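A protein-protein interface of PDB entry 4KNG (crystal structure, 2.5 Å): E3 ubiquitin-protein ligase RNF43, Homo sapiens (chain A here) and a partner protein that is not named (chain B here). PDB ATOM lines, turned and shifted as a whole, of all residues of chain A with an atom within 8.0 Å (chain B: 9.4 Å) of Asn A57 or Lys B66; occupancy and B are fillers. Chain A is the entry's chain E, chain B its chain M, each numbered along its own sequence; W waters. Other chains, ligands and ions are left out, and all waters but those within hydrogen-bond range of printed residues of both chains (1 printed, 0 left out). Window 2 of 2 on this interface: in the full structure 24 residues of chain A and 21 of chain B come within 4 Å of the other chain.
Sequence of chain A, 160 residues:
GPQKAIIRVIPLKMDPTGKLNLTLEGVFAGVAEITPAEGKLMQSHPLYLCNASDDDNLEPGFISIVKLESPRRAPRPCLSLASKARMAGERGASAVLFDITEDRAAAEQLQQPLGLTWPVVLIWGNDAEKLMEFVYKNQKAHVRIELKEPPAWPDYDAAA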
ATOM      1  N   TYR A  48      31.840 -32.490 -14.617  1.00  0.00           N
ATOM      2  CA  TYR A  48      31.771 -31.653 -13.445  1.00  0.00           C
ATOM      3  C   TYR A  48      32.683 -30.475 -13.630  1.00  0.00           C
ATOM      4  O   TYR A  48      32.312 -29.352 -13.308  1.00  0.00           O
ATOM      5  CB  TYR A  48      32.127 -32.433 -12.187  1.00  0.00           C
ATOM      6  CG  TYR A  48      32.198 -31.616 -10.917  1.00  0.00           C
ATOM      7  CD1 TYR A  48      31.076 -31.395 -10.150  1.00  0.00           C
ATOM      8  CD2 TYR A  48      33.418 -31.115 -10.456  1.00  0.00           C
ATOM      9  CE1 TYR A  48      31.147 -30.679  -8.983  1.00  0.00           C
ATOM     10  CE2 TYR A  48      33.508 -30.402  -9.284  1.00  0.00           C
ATOM     11  CZ  TYR A  48      32.370 -30.182  -8.554  1.00  0.00           C
ATOM     12  OH  TYR A  48      32.459 -29.451  -7.403  1.00  0.00           O
ATOM     13  N   SER A  53      29.391 -25.546 -13.954  1.00  0.00           N
ATOM     14  CA  SER A  53      28.553 -26.524 -13.253  1.00  0.00           C
ATOM     15  C   SER A  53      28.444 -26.206 -11.765  1.00  0.00           C
ATOM     16  O   SER A  53      29.142 -25.331 -11.245  1.00  0.00           O
ATOM     17  CB  SER A  53      29.131 -27.925 -13.417  1.00  0.00           C
ATOM     18  OG  SER A  53      28.970 -28.374 -14.741  1.00  0.00           O
ATOM     19  N   ASP A  54      27.573 -26.929 -11.078  1.00  0.00           N
ATOM     20  CA  ASP A  54      27.370 -26.714  -9.648  1.00  0.00           C
ATOM     21  C   ASP A  54      28.536 -27.260  -8.816  1.00  0.00           C
ATOM     22  O   ASP A  54      28.831 -28.455  -8.853  1.00  0.00           O
ATOM     23  CB  ASP A  54      26.051 -27.345  -9.212  1.00  0.00           C
ATOM     24  CG  ASP A  54      24.862 -26.803  -9.996  1.00  0.00           C
ATOM     25  OD1 ASP A  54      24.782 -25.575 -10.174  1.00  0.00           O
ATOM     26  OD2 ASP A  54      24.016 -27.602 -10.455  1.00  0.00           O
ATOM     27  N   ASP A  55      29.202 -26.370  -8.083  1.00  0.00           N
ATOM     28  CA  ASP A  55      30.212 -26.765  -7.113  1.00  0.00           C
ATOM     29  C   ASP A  55      29.551 -27.675  -6.081  1.00  0.00           C
ATOM     30  O   ASP A  55      28.503 -27.355  -5.549  1.00  0.00           O
ATOM     31  CB  ASP A  55      30.797 -25.515  -6.455  1.00  0.00           C
ATOM     32  CG  ASP A  55      32.012 -25.799  -5.611  1.00  0.00           C
ATOM     33  OD1 ASP A  55      32.063 -26.855  -4.965  1.00  0.00           O
ATOM     34  OD2 ASP A  55      32.911 -24.941  -5.559  1.00  0.00           O
ATOM     35  N   ASP A  56      30.132 -28.841  -5.845  1.00  0.00           N
ATOM     36  CA  ASP A  56      29.616 -29.770  -4.844  1.00  0.00           C
ATOM     37  C   ASP A  56      29.893 -29.267  -3.418  1.00  0.00           C
ATOM     38  O   ASP A  56      29.309 -29.761  -2.441  1.00  0.00           O
ATOM     39  CB  ASP A  56      30.264 -31.158  -5.013  1.00  0.00           C
ATOM     40  CG  ASP A  56      29.476 -32.091  -5.887  1.00  0.00           C
ATOM     41  OD1 ASP A  56      28.229 -31.980  -5.908  1.00  0.00           O
ATOM     42  OD2 ASP A  56      30.125 -32.966  -6.509  1.00  0.00           O
ATOM     43  N   ASN A  57      30.809 -28.313  -3.306  1.00  0.00           N
ATOM     44  CA  ASN A  57      31.183 -27.718  -2.026  1.00  0.00           C
ATOM     45  C   ASN A  57      31.636 -28.762  -1.010  1.00  0.00           C
ATOM     46  O   ASN A  57      31.078 -28.884   0.074  1.00  0.00           O
ATOM     47  CB  ASN A  57      30.056 -26.843  -1.477  1.00  0.00           C
ATOM     48  CG  ASN A  57      29.810 -25.620  -2.341  1.00  0.00           C
ATOM     49  OD1 ASN A  57      30.695 -24.758  -2.506  1.00  0.00           O
ATOM     50  ND2 ASN A  57      28.617 -25.540  -2.918  1.00  0.00           N
ATOM     51  N   LEU A  58      32.659 -29.516  -1.404  1.00  0.00           N
ATOM     52  CA  LEU A  58      33.313 -30.463  -0.522  1.00  0.00           C
ATOM     53  C   LEU A  58      34.219 -29.682   0.409  1.00  0.00           C
ATOM     54  O   LEU A  58      34.591 -28.520   0.152  1.00  0.00           O
ATOM     55  CB  LEU A  58      34.175 -31.457  -1.312  1.00  0.00           C
ATOM     56  CG  LEU A  58      33.525 -32.598  -2.094  1.00  0.00           C
ATOM     57  CD1 LEU A  58      32.145 -32.240  -2.604  1.00  0.00           C
ATOM     58  CD2 LEU A  58      34.428 -33.024  -3.253  1.00  0.00           C
ATOM     59  N   GLU A  59      34.581 -30.334   1.498  1.00  0.00           N
ATOM     60  CA  GLU A  59      35.531 -29.732   2.384  1.00  0.00           C
ATOM     61  C   GLU A  59      36.871 -29.695   1.671  1.00  0.00           C
ATOM     62  O   GLU A  59      37.422 -30.755   1.339  1.00  0.00           O
ATOM     63  CB  GLU A  59      35.643 -30.486   3.702  1.00  0.00           C
ATOM     64  CG  GLU A  59      36.381 -29.658   4.743  1.00  0.00           C
ATOM     65  CD  GLU A  59      35.481 -28.626   5.409  1.00  0.00           C
ATOM     66  OE1 GLU A  59      35.830 -27.412   5.389  1.00  0.00           O
ATOM     67  OE2 GLU A  59      34.419 -29.047   5.948  1.00  0.00           O
ATOM     68  N   PRO A  60      37.402 -28.481   1.442  1.00  0.00           N
ATOM     69  CA  PRO A  60      38.673 -28.339   0.733  1.00  0.00           C
ATOM     70  C   PRO A  60      39.775 -29.244   1.280  1.00  0.00           C
ATOM     71  O   PRO A  60      39.809 -29.524   2.474  1.00  0.00           O
ATOM     72  CB  PRO A  60      39.037 -26.859   0.935  1.00  0.00           C
ATOM     73  CG  PRO A  60      37.723 -26.191   1.200  1.00  0.00           C
ATOM     74  CD  PRO A  60      36.904 -27.192   1.952  1.00  0.00           C
ATOM     75  N   PHE A  62      40.617 -32.392  -0.241  1.00  0.00           N
ATOM     76  CA  PHE A  62      40.463 -33.698  -0.923  1.00  0.00           C
ATOM     77  C   PHE A  62      41.255 -33.771  -2.207  1.00  0.00           C
ATOM     78  O   PHE A  62      41.655 -32.747  -2.772  1.00  0.00           O
ATOM     79  CB  PHE A  62      39.004 -33.949  -1.286  1.00  0.00           C
ATOM     80  CG  PHE A  62      38.471 -32.950  -2.283  1.00  0.00           C
ATOM     81  CD1 PHE A  62      38.046 -31.674  -1.875  1.00  0.00           C
ATOM     82  CD2 PHE A  62      38.426 -33.259  -3.634  1.00  0.00           C
ATOM     83  CE1 PHE A  62      37.589 -30.750  -2.792  1.00  0.00           C
ATOM     84  CE2 PHE A  62      37.964 -32.336  -4.548  1.00  0.00           C
ATOM     85  CZ  PHE A  62      37.548 -31.085  -4.130  1.00  0.00           C
ATOM     86  N   ARG A  91      38.128 -25.136  -6.699  1.00  0.00           N
ATOM     87  CA  ARG A  91      36.983 -25.732  -6.052  1.00  0.00           C
ATOM     88  C   ARG A  91      37.308 -26.612  -4.862  1.00  0.00           C
ATOM     89  O   ARG A  91      36.409 -27.267  -4.347  1.00  0.00           O
ATOM     90  CB  ARG A  91      36.181 -26.550  -7.089  1.00  0.00           C
ATOM     91  CG  ARG A  91      35.254 -25.695  -7.902  1.00  0.00           C
ATOM     92  CD  ARG A  91      34.130 -26.514  -8.477  1.00  0.00           C
ATOM     93  NE  ARG A  91      33.374 -25.716  -9.406  1.00  0.00           N
ATOM     94  CZ  ARG A  91      32.456 -26.204 -10.222  1.00  0.00           C
ATOM     95  NH1 ARG A  91      32.163 -27.497 -10.222  1.00  0.00           N
ATOM     96  NH2 ARG A  91      31.850 -25.385 -11.055  1.00  0.00           N
ATOM     97  N   GLY A  92      38.567 -26.676  -4.436  1.00  0.00           N
ATOM     98  CA  GLY A  92      38.875 -27.343  -3.184  1.00  0.00           C
ATOM     99  C   GLY A  92      39.994 -28.359  -3.209  1.00  0.00           C
ATOM    100  O   GLY A  92      40.518 -28.710  -2.153  1.00  0.00           O
ATOM    101  N   ARG B  34      26.341 -37.667  -7.171  1.00  0.00           N
ATOM    102  CA  ARG B  34      27.438 -38.035  -6.268  1.00  0.00           C
ATOM    103  C   ARG B  34      27.008 -38.967  -5.159  1.00  0.00           C
ATOM    104  O   ARG B  34      25.981 -38.731  -4.542  1.00  0.00           O
ATOM    105  CB  ARG B  34      28.055 -36.807  -5.598  1.00  0.00           C
ATOM    106  CG  ARG B  34      29.225 -37.192  -4.706  1.00  0.00           C
ATOM    107  CD  ARG B  34      30.103 -36.018  -4.352  1.00  0.00           C
ATOM    108  NE  ARG B  34      31.041 -35.629  -5.415  1.00  0.00           N
ATOM    109  CZ  ARG B  34      32.052 -36.371  -5.856  1.00  0.00           C
ATOM    110  NH1 ARG B  34      32.273 -37.577  -5.363  1.00  0.00           N
ATOM    111  NH2 ARG B  34      32.838 -35.908  -6.823  1.00  0.00           N
ATOM    112  N   GLN B  39      31.071 -40.069  -8.546  1.00  0.00           N
ATOM    113  CA  GLN B  39      30.277 -39.104  -9.281  1.00  0.00           C
ATOM    114  C   GLN B  39      29.988 -39.697 -10.653  1.00  0.00           C
ATOM    115  O   GLN B  39      30.897 -39.887 -11.492  1.00  0.00           O
ATOM    116  CB  GLN B  39      30.992 -37.762  -9.428  1.00  0.00           C
ATOM    117  CG  GLN B  39      30.047 -36.653  -9.827  1.00  0.00           C
ATOM    118  CD  GLN B  39      30.720 -35.326  -9.980  1.00  0.00           C
ATOM    119  OE1 GLN B  39      31.744 -35.191 -10.668  1.00  0.00           O
ATOM    120  NE2 GLN B  39      30.164 -34.314  -9.317  1.00  0.00           N
ATOM    121  N   PRO B  49      13.999 -32.341  -7.518  1.00  0.00           N
ATOM    122  CA  PRO B  49      13.753 -31.246  -6.559  1.00  0.00           C
ATOM    123  C   PRO B  49      14.817 -30.170  -6.302  1.00  0.00           C
ATOM    124  O   PRO B  49      14.562 -28.955  -6.441  1.00  0.00           O
ATOM    125  CB  PRO B  49      13.478 -32.024  -5.310  1.00  0.00           C
ATOM    126  CG  PRO B  49      12.570 -33.120  -5.857  1.00  0.00           C
ATOM    127  CD  PRO B  49      13.129 -33.493  -7.201  1.00  0.00           C
ATOM    128  N   GLY B  50      16.026 -30.545  -5.971  1.00  0.00           N
ATOM    129  CA  GLY B  50      17.034 -29.478  -5.907  1.00  0.00           C
ATOM    130  C   GLY B  50      17.190 -28.613  -7.179  1.00  0.00           C
ATOM    131  O   GLY B  50      17.851 -27.567  -7.141  1.00  0.00           O
ATOM    132  N   TYR B  51      16.591 -29.020  -8.302  1.00  0.00           N
ATOM    133  CA  TYR B  51      17.077 -28.596  -9.607  1.00  0.00           C
ATOM    134  C   TYR B  51      16.028 -28.054 -10.546  1.00  0.00           C
ATOM    135  O   TYR B  51      14.845 -28.302 -10.403  1.00  0.00           O
ATOM    136  CB  TYR B  51      17.707 -29.792 -10.299  1.00  0.00           C
ATOM    137  CG  TYR B  51      18.855 -30.422  -9.530  1.00  0.00           C
ATOM    138  CD1 TYR B  51      18.624 -31.419  -8.565  1.00  0.00           C
ATOM    139  CD2 TYR B  51      20.160 -30.021  -9.765  1.00  0.00           C
ATOM    140  CE1 TYR B  51      19.662 -31.988  -7.860  1.00  0.00           C
ATOM    141  CE2 TYR B  51      21.202 -30.577  -9.065  1.00  0.00           C
ATOM    142  CZ  TYR B  51      20.956 -31.556  -8.118  1.00  0.00           C
ATOM    143  OH  TYR B  51      22.026 -32.104  -7.445  1.00  0.00           O
ATOM    144  N   PHE B  52      16.495 -27.351 -11.554  1.00  0.00           N
ATOM    145  CA  PHE B  52      15.703 -27.085 -12.736  1.00  0.00           C
ATOM    146  C   PHE B  52      16.303 -27.620 -14.073  1.00  0.00           C
ATOM    147  O   PHE B  52      17.509 -27.762 -14.248  1.00  0.00           O
ATOM    148  CB  PHE B  52      15.449 -25.599 -12.845  1.00  0.00           C
ATOM    149  CG  PHE B  52      16.664 -24.770 -13.109  1.00  0.00           C
ATOM    150  CD1 PHE B  52      17.467 -24.338 -12.081  1.00  0.00           C
ATOM    151  CD2 PHE B  52      16.951 -24.354 -14.389  1.00  0.00           C
ATOM    152  CE1 PHE B  52      18.546 -23.508 -12.325  1.00  0.00           C
ATOM    153  CE2 PHE B  52      18.036 -23.530 -14.647  1.00  0.00           C
ATOM    154  CZ  PHE B  52      18.832 -23.110 -13.617  1.00  0.00           C
ATOM    155  N   ILE B  63      20.295 -28.398 -13.295  1.00  0.00           N
ATOM    156  CA  ILE B  63      21.044 -27.348 -12.644  1.00  0.00           C
ATOM    157  C   ILE B  63      20.470 -27.051 -11.267  1.00  0.00           C
ATOM    158  O   ILE B  63      19.261 -27.020 -11.072  1.00  0.00           O
ATOM    159  CB  ILE B  63      21.091 -26.084 -13.491  1.00  0.00           C
ATOM    160  CG1 ILE B  63      21.962 -26.362 -14.695  1.00  0.00           C
ATOM    161  CG2 ILE B  63      21.669 -24.930 -12.699  1.00  0.00           C
ATOM    162  CD1 ILE B  63      22.021 -25.227 -15.687  1.00  0.00           C
ATOM    163  N   LYS B  64      21.358 -26.843 -10.310  1.00  0.00           N
ATOM    164  CA  LYS B  64      20.953 -26.790  -8.924  1.00  0.00           C
ATOM    165  C   LYS B  64      20.335 -25.427  -8.657  1.00  0.00           C
ATOM    166  O   LYS B  64      20.894 -24.380  -8.999  1.00  0.00           O
ATOM    167  CB  LYS B  64      22.114 -27.079  -7.964  1.00  0.00           C
ATOM    168  CG  LYS B  64      21.661 -27.660  -6.640  1.00  0.00           C
ATOM    169  CD  LYS B  64      22.796 -27.770  -5.648  1.00  0.00           C
ATOM    170  CE  LYS B  64      23.822 -28.811  -6.064  1.00  0.00           C
ATOM    171  NZ  LYS B  64      25.095 -28.625  -5.310  1.00  0.00           N
ATOM    172  N   CYS B  65      19.134 -25.481  -8.096  1.00  0.00           N
ATOM    173  CA  CYS B  65      18.377 -24.315  -7.710  1.00  0.00           C
ATOM    174  C   CYS B  65      18.997 -23.709  -6.456  1.00  0.00           C
ATOM    175  O   CYS B  65      18.821 -24.228  -5.379  1.00  0.00           O
ATOM    176  CB  CYS B  65      16.945 -24.770  -7.434  1.00  0.00           C
ATOM    177  SG  CYS B  65      15.799 -23.400  -7.482  1.00  0.00           S
ATOM    178  N   LYS B  66      19.753 -22.633  -6.581  1.00  0.00           N
ATOM    179  CA  LYS B  66      20.596 -22.218  -5.449  1.00  0.00           C
ATOM    180  C   LYS B  66      19.925 -21.245  -4.497  1.00  0.00           C
ATOM    181  O   LYS B  66      20.382 -21.104  -3.353  1.00  0.00           O
ATOM    182  CB  LYS B  66      21.951 -21.659  -5.937  1.00  0.00           C
ATOM    183  CG  LYS B  66      23.055 -22.710  -6.020  1.00  0.00           C
ATOM    184  CD  LYS B  66      23.661 -23.006  -4.653  1.00  0.00           C
ATOM    185  CE  LYS B  66      24.822 -23.987  -4.749  1.00  0.00           C
ATOM    186  NZ  LYS B  66      25.457 -24.195  -3.418  1.00  0.00           N
ATOM    187  N   ILE B  67      18.825 -20.629  -4.943  1.00  0.00           N
ATOM    188  CA  ILE B  67      18.332 -19.380  -4.352  1.00  0.00           C
ATOM    189  C   ILE B  67      17.566 -19.524  -3.038  1.00  0.00           C
ATOM    190  O   ILE B  67      16.641 -20.327  -2.913  1.00  0.00           O
ATOM    191  CB  ILE B  67      17.536 -18.495  -5.353  1.00  0.00           C
ATOM    192  CG1 ILE B  67      16.412 -19.231  -6.098  1.00  0.00           C
ATOM    193  CG2 ILE B  67      18.500 -17.841  -6.330  1.00  0.00           C
ATOM    194  CD1 ILE B  67      15.695 -18.407  -7.161  1.00  0.00           C
ATOM    195  N   GLU B  68      18.022 -18.711  -2.077  1.00  0.00           N
ATOM    196  CA  GLU B  68      17.507 -18.570  -0.691  1.00  0.00           C
ATOM    197  C   GLU B  68      16.040 -18.943  -0.424  1.00  0.00           C
ATOM    198  O   GLU B  68      15.124 -18.213  -0.770  1.00  0.00           O
ATOM    199  CB  GLU B  68      17.778 -17.137  -0.146  1.00  0.00           C
ATOM    200  CG  GLU B  68      17.839 -15.989  -1.183  1.00  0.00           C
ATOM    201  CD  GLU B  68      16.522 -15.228  -1.406  1.00  0.00           C
ATOM    202  OE1 GLU B  68      15.451 -15.850  -1.579  1.00  0.00           O
ATOM    203  OE2 GLU B  68      16.562 -13.974  -1.437  1.00  0.00           O
ATOM    204  N   HIS B  69      15.846 -20.068   0.248  1.00  0.00           N
ATOM    205  CA  HIS B  69      14.525 -20.510   0.706  1.00  0.00           C
ATOM    206  C   HIS B  69      13.633 -20.987  -0.425  1.00  0.00           C
ATOM    207  O   HIS B  69      12.434 -21.085  -0.222  1.00  0.00           O
ATOM    208  CB  HIS B  69      13.759 -19.424   1.500  1.00  0.00           C
ATOM    209  CG  HIS B  69      14.614 -18.600   2.425  1.00  0.00           C
ATOM    210  ND1 HIS B  69      14.566 -17.218   2.450  1.00  0.00           N
ATOM    211  CD2 HIS B  69      15.544 -18.959   3.345  1.00  0.00           C
ATOM    212  CE1 HIS B  69      15.431 -16.763   3.337  1.00  0.00           C
ATOM    213  NE2 HIS B  69      16.041 -17.798   3.889  1.00  0.00           N
ATOM    214  N   CYS B  70      14.206 -21.299  -1.596  1.00  0.00           N
ATOM    215  CA  CYS B  70      13.421 -21.763  -2.743  1.00  0.00           C
ATOM    216  C   CYS B  70      13.395 -23.272  -2.802  1.00  0.00           C
ATOM    217  O   CYS B  70      14.400 -23.903  -2.568  1.00  0.00           O
ATOM    218  CB  CYS B  70      13.972 -21.196  -4.058  1.00  0.00           C
ATOM    219  SG  CYS B  70      12.875 -21.515  -5.460  1.00  0.00           S
ATOM    220  N   GLU B  71      12.239 -23.846  -3.102  1.00  0.00           N
ATOM    221  CA  GLU B  71      12.082 -25.276  -3.280  1.00  0.00           C
ATOM    222  C   GLU B  71      12.001 -25.659  -4.746  1.00  0.00           C
ATOM    223  O   GLU B  71      12.172 -26.828  -5.080  1.00  0.00           O
ATOM    224  CB  GLU B  71      10.754 -25.763  -2.696  1.00  0.00           C
ATOM    225  CG  GLU B  71      10.595 -25.870  -1.178  1.00  0.00           C
ATOM    226  CD  GLU B  71       9.307 -26.633  -0.766  1.00  0.00           C
ATOM    227  OE1 GLU B  71       8.644 -27.284  -1.625  1.00  0.00           O
ATOM    228  OE2 GLU B  71       8.943 -26.586   0.431  1.00  0.00           O
ATOM    229  N   ALA B  72      11.610 -24.725  -5.613  1.00  0.00           N
ATOM    230  CA  ALA B  72      11.496 -25.020  -7.033  1.00  0.00           C
ATOM    231  C   ALA B  72      11.641 -23.759  -7.862  1.00  0.00           C
ATOM    232  O   ALA B  72      10.891 -22.810  -7.676  1.00  0.00           O
ATOM    233  CB  ALA B  72      10.163 -25.681  -7.317  1.00  0.00           C
ATOM    234  N   CYS B  73      12.593 -23.743  -8.784  1.00  0.00           N
ATOM    235  CA  CYS B  73      12.753 -22.573  -9.619  1.00  0.00           C
ATOM    236  C   CYS B  73      12.558 -22.847 -11.070  1.00  0.00           C
ATOM    237  O   CYS B  73      12.582 -23.986 -11.536  1.00  0.00           O
ATOM    238  CB  CYS B  73      14.117 -21.926  -9.443  1.00  0.00           C
ATOM    239  SG  CYS B  73      15.441 -23.107  -9.462  1.00  0.00           S
ATOM    240  N   PHE B  74      12.402 -21.742 -11.773  1.00  0.00           N
ATOM    241  CA  PHE B  74      12.240 -21.737 -13.199  1.00  0.00           C
ATOM    242  C   PHE B  74      13.619 -21.641 -13.827  1.00  0.00           C
ATOM    243  O   PHE B  74      13.935 -22.346 -14.761  1.00  0.00           O
ATOM    244  CB  PHE B  74      11.403 -20.540 -13.568  1.00  0.00           C
ATOM    245  CG  PHE B  74      11.459 -20.171 -15.009  1.00  0.00           C
ATOM    246  CD1 PHE B  74      12.405 -19.294 -15.473  1.00  0.00           C
ATOM    247  CD2 PHE B  74      10.554 -20.691 -15.887  1.00  0.00           C
ATOM    248  CE1 PHE B  74      12.430 -18.943 -16.806  1.00  0.00           C
ATOM    249  CE2 PHE B  74      10.567 -20.344 -17.204  1.00  0.00           C
ATOM    250  CZ  PHE B  74      11.513 -19.481 -17.674  1.00  0.00           C
ATOM    251  N   SER B  75      14.427 -20.774 -13.255  1.00  0.00           N
ATOM    252  CA  SER B  75      15.815 -20.626 -13.618  1.00  0.00           C
ATOM    253  C   SER B  75      16.594 -20.286 -12.390  1.00  0.00           C
ATOM    254  O   SER B  75      16.051 -20.229 -11.285  1.00  0.00           O
ATOM    255  CB  SER B  75      15.937 -19.481 -14.574  1.00  0.00           C
ATOM    256  OG  SER B  75      15.470 -18.308 -13.967  1.00  0.00           O
ATOM    257  N   HIS B  76      17.886 -20.041 -12.566  1.00  0.00           N
ATOM    258  CA  HIS B  76      18.791 -19.997 -11.429  1.00  0.00           C
ATOM    259  C   HIS B  76      18.377 -18.857 -10.548  1.00  0.00           C
ATOM    260  O   HIS B  76      18.453 -18.922  -9.354  1.00  0.00           O
ATOM    261  CB  HIS B  76      20.233 -19.838 -11.897  1.00  0.00           C
ATOM    262  CG  HIS B  76      20.594 -18.442 -12.295  1.00  0.00           C
ATOM    263  ND1 HIS B  76      20.456 -17.978 -13.585  1.00  0.00           N
ATOM    264  CD2 HIS B  76      21.117 -17.416 -11.581  1.00  0.00           C
ATOM    265  CE1 HIS B  76      20.877 -16.723 -13.652  1.00  0.00           C
ATOM    266  NE2 HIS B  76      21.264 -16.351 -12.445  1.00  0.00           N
ATOM    267  N   ASN B  77      17.866 -17.836 -11.203  1.00  0.00           N
ATOM    268  CA  ASN B  77      17.461 -16.563 -10.634  1.00  0.00           C
ATOM    269  C   ASN B  77      16.050 -16.487 -10.139  1.00  0.00           C
ATOM    270  O   ASN B  77      15.715 -15.532  -9.501  1.00  0.00           O
ATOM    271  CB  ASN B  77      17.464 -15.554 -11.788  1.00  0.00           C
ATOM    272  CG  ASN B  77      18.490 -14.503 -11.625  1.00  0.00           C
ATOM    273  OD1 ASN B  77      19.044 -14.319 -10.539  1.00  0.00           O
ATOM    274  ND2 ASN B  77      18.751 -13.781 -12.700  1.00  0.00           N
ATOM    275  N   PHE B  78      15.188 -17.408 -10.523  1.00  0.00           N
ATOM    276  CA  PHE B  78      13.747 -17.142 -10.418  1.00  0.00           C
ATOM    277  C   PHE B  78      13.005 -18.309  -9.862  1.00  0.00           C
ATOM    278  O   PHE B  78      12.820 -19.349 -10.530  1.00  0.00           O
ATOM    279  CB  PHE B  78      13.164 -16.823 -11.759  1.00  0.00           C
ATOM    280  CG  PHE B  78      11.772 -16.342 -11.693  1.00  0.00           C
ATOM    281  CD1 PHE B  78      10.735 -17.222 -11.612  1.00  0.00           C
ATOM    282  CD2 PHE B  78      11.495 -15.007 -11.732  1.00  0.00           C
ATOM    283  CE1 PHE B  78       9.436 -16.783 -11.561  1.00  0.00           C
ATOM    284  CE2 PHE B  78      10.198 -14.545 -11.679  1.00  0.00           C
ATOM    285  CZ  PHE B  78       9.168 -15.435 -11.614  1.00  0.00           C
ATOM    286  N   CYS B  79      12.610 -18.107  -8.610  1.00  0.00           N
ATOM    287  CA  CYS B  79      11.927 -19.104  -7.825  1.00  0.00           C
ATOM    288  C   CYS B  79      10.439 -19.201  -8.192  1.00  0.00           C
ATOM    289  O   CYS B  79       9.814 -18.211  -8.531  1.00  0.00           O
ATOM    290  CB  CYS B  79      12.080 -18.745  -6.353  1.00  0.00           C
ATOM    291  SG  CYS B  79      11.420 -20.049  -5.358  1.00  0.00           S
ATOM    292  N   CYS B  93      12.280 -14.916  -2.671  1.00  0.00           N
ATOM    293  CA  CYS B  93      11.616 -15.303  -1.418  1.00  0.00           C
ATOM    294  C   CYS B  93      11.893 -14.331  -0.253  1.00  0.00           C
ATOM    295  O   CYS B  93      13.062 -14.064   0.104  1.00  0.00           O
ATOM    296  CB  CYS B  93      12.086 -16.681  -0.984  1.00  0.00           C
ATOM    297  SG  CYS B  93      11.628 -18.058  -2.042  1.00  0.00           S
HETATM  298  O   HOH W   1      32.909 -33.295  -7.892  1.00  0.00           O
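Of the 24 printed residues of chain B, 5 touch a printed residue of chain A.
Hydrophobic or aromatic side chains of chain A within 4 Å of the printed part of chain B: Tyr A48.
Among the printed residues, Asp or Glu carboxylates within 4 Å of a Lys or Arg side-chain nitrogen of the other chain: Asp A56 with Arg B34.
Gln B39 touches Tyr A48 (NE2 to CD1, 3.2 Å).
Asp A54 touches Ile B63 (OD2 to C, 3.7 Å).
Lys B64 touches Asp A55 (NZ to O, 3.6 Å).
ND2 of Asn A57 lies close to NZ of Lys B66, 3.5 Å away.
The side-chain carboxylate (OD2) of Asp A56 lies within salt-bridge range of the guanidinium group (NE) of Arg B34 (3.0 Å).
The backbone NH (N) of Lys B64 lies within hydrogen-bond range of the side-chain carboxylate (OD2) of Asp A54 (2.8 Å).
NE2 of Gln B39 is in hydrogen-bond range of OD2 of Asp A56.
Water W1 lies within hydrogen-bond range of NH2 of Arg B34, OD2 of Asp A56 and NE2 of Gln B39.
Printed residues of chain B within 4 Å of Asp A55: Lys B64.
Of the printed residues of chain B, Asp A56 touches Arg B34 and Gln B39.
Of chain B, only Lys B66 comes within 4 Å of Asn A57.
Printed residues of chain A within 4 Å of Lys B64: Asp A54 and Asp A55.
Lys B66 touches just one residue of chain A: Asn A57 (3.5 Å).
His B69 touches none of the printed residues of chain A.
Phe B78 touches none of the printed residues of chain A.
The nearest residue of chain B that does not touch Asn A57 is Lys B64 (5.3 Å).
The backbone NH (N) of Phe B52 sits at hydrogen-bond distance from the backbone carbonyl oxygen (O) of Ile B63, at 2.8 Å.
The guanidinium group of Arg A91 lies within salt-bridge range of the side-chain carboxylate of Asp A55, 3.95 Å away.
SG of Cys B70 is disulfide-bonded to SG of Cys B79 (2.1 Å).
The backbone NH (N) of Asn A57 sits at hydrogen-bond distance from the side-chain carboxylate (OD1) of Asp A55 (2.5 Å).
The side-chain hydroxyl (OH) of Tyr A48 is in hydrogen-bond range of the backbone NH (N) of Asp A56.
The side-chain sulfur (SG) of Cys B65 is disulfide-bonded to the side-chain sulfur (SG) of Cys B73, 2.0 Å away.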
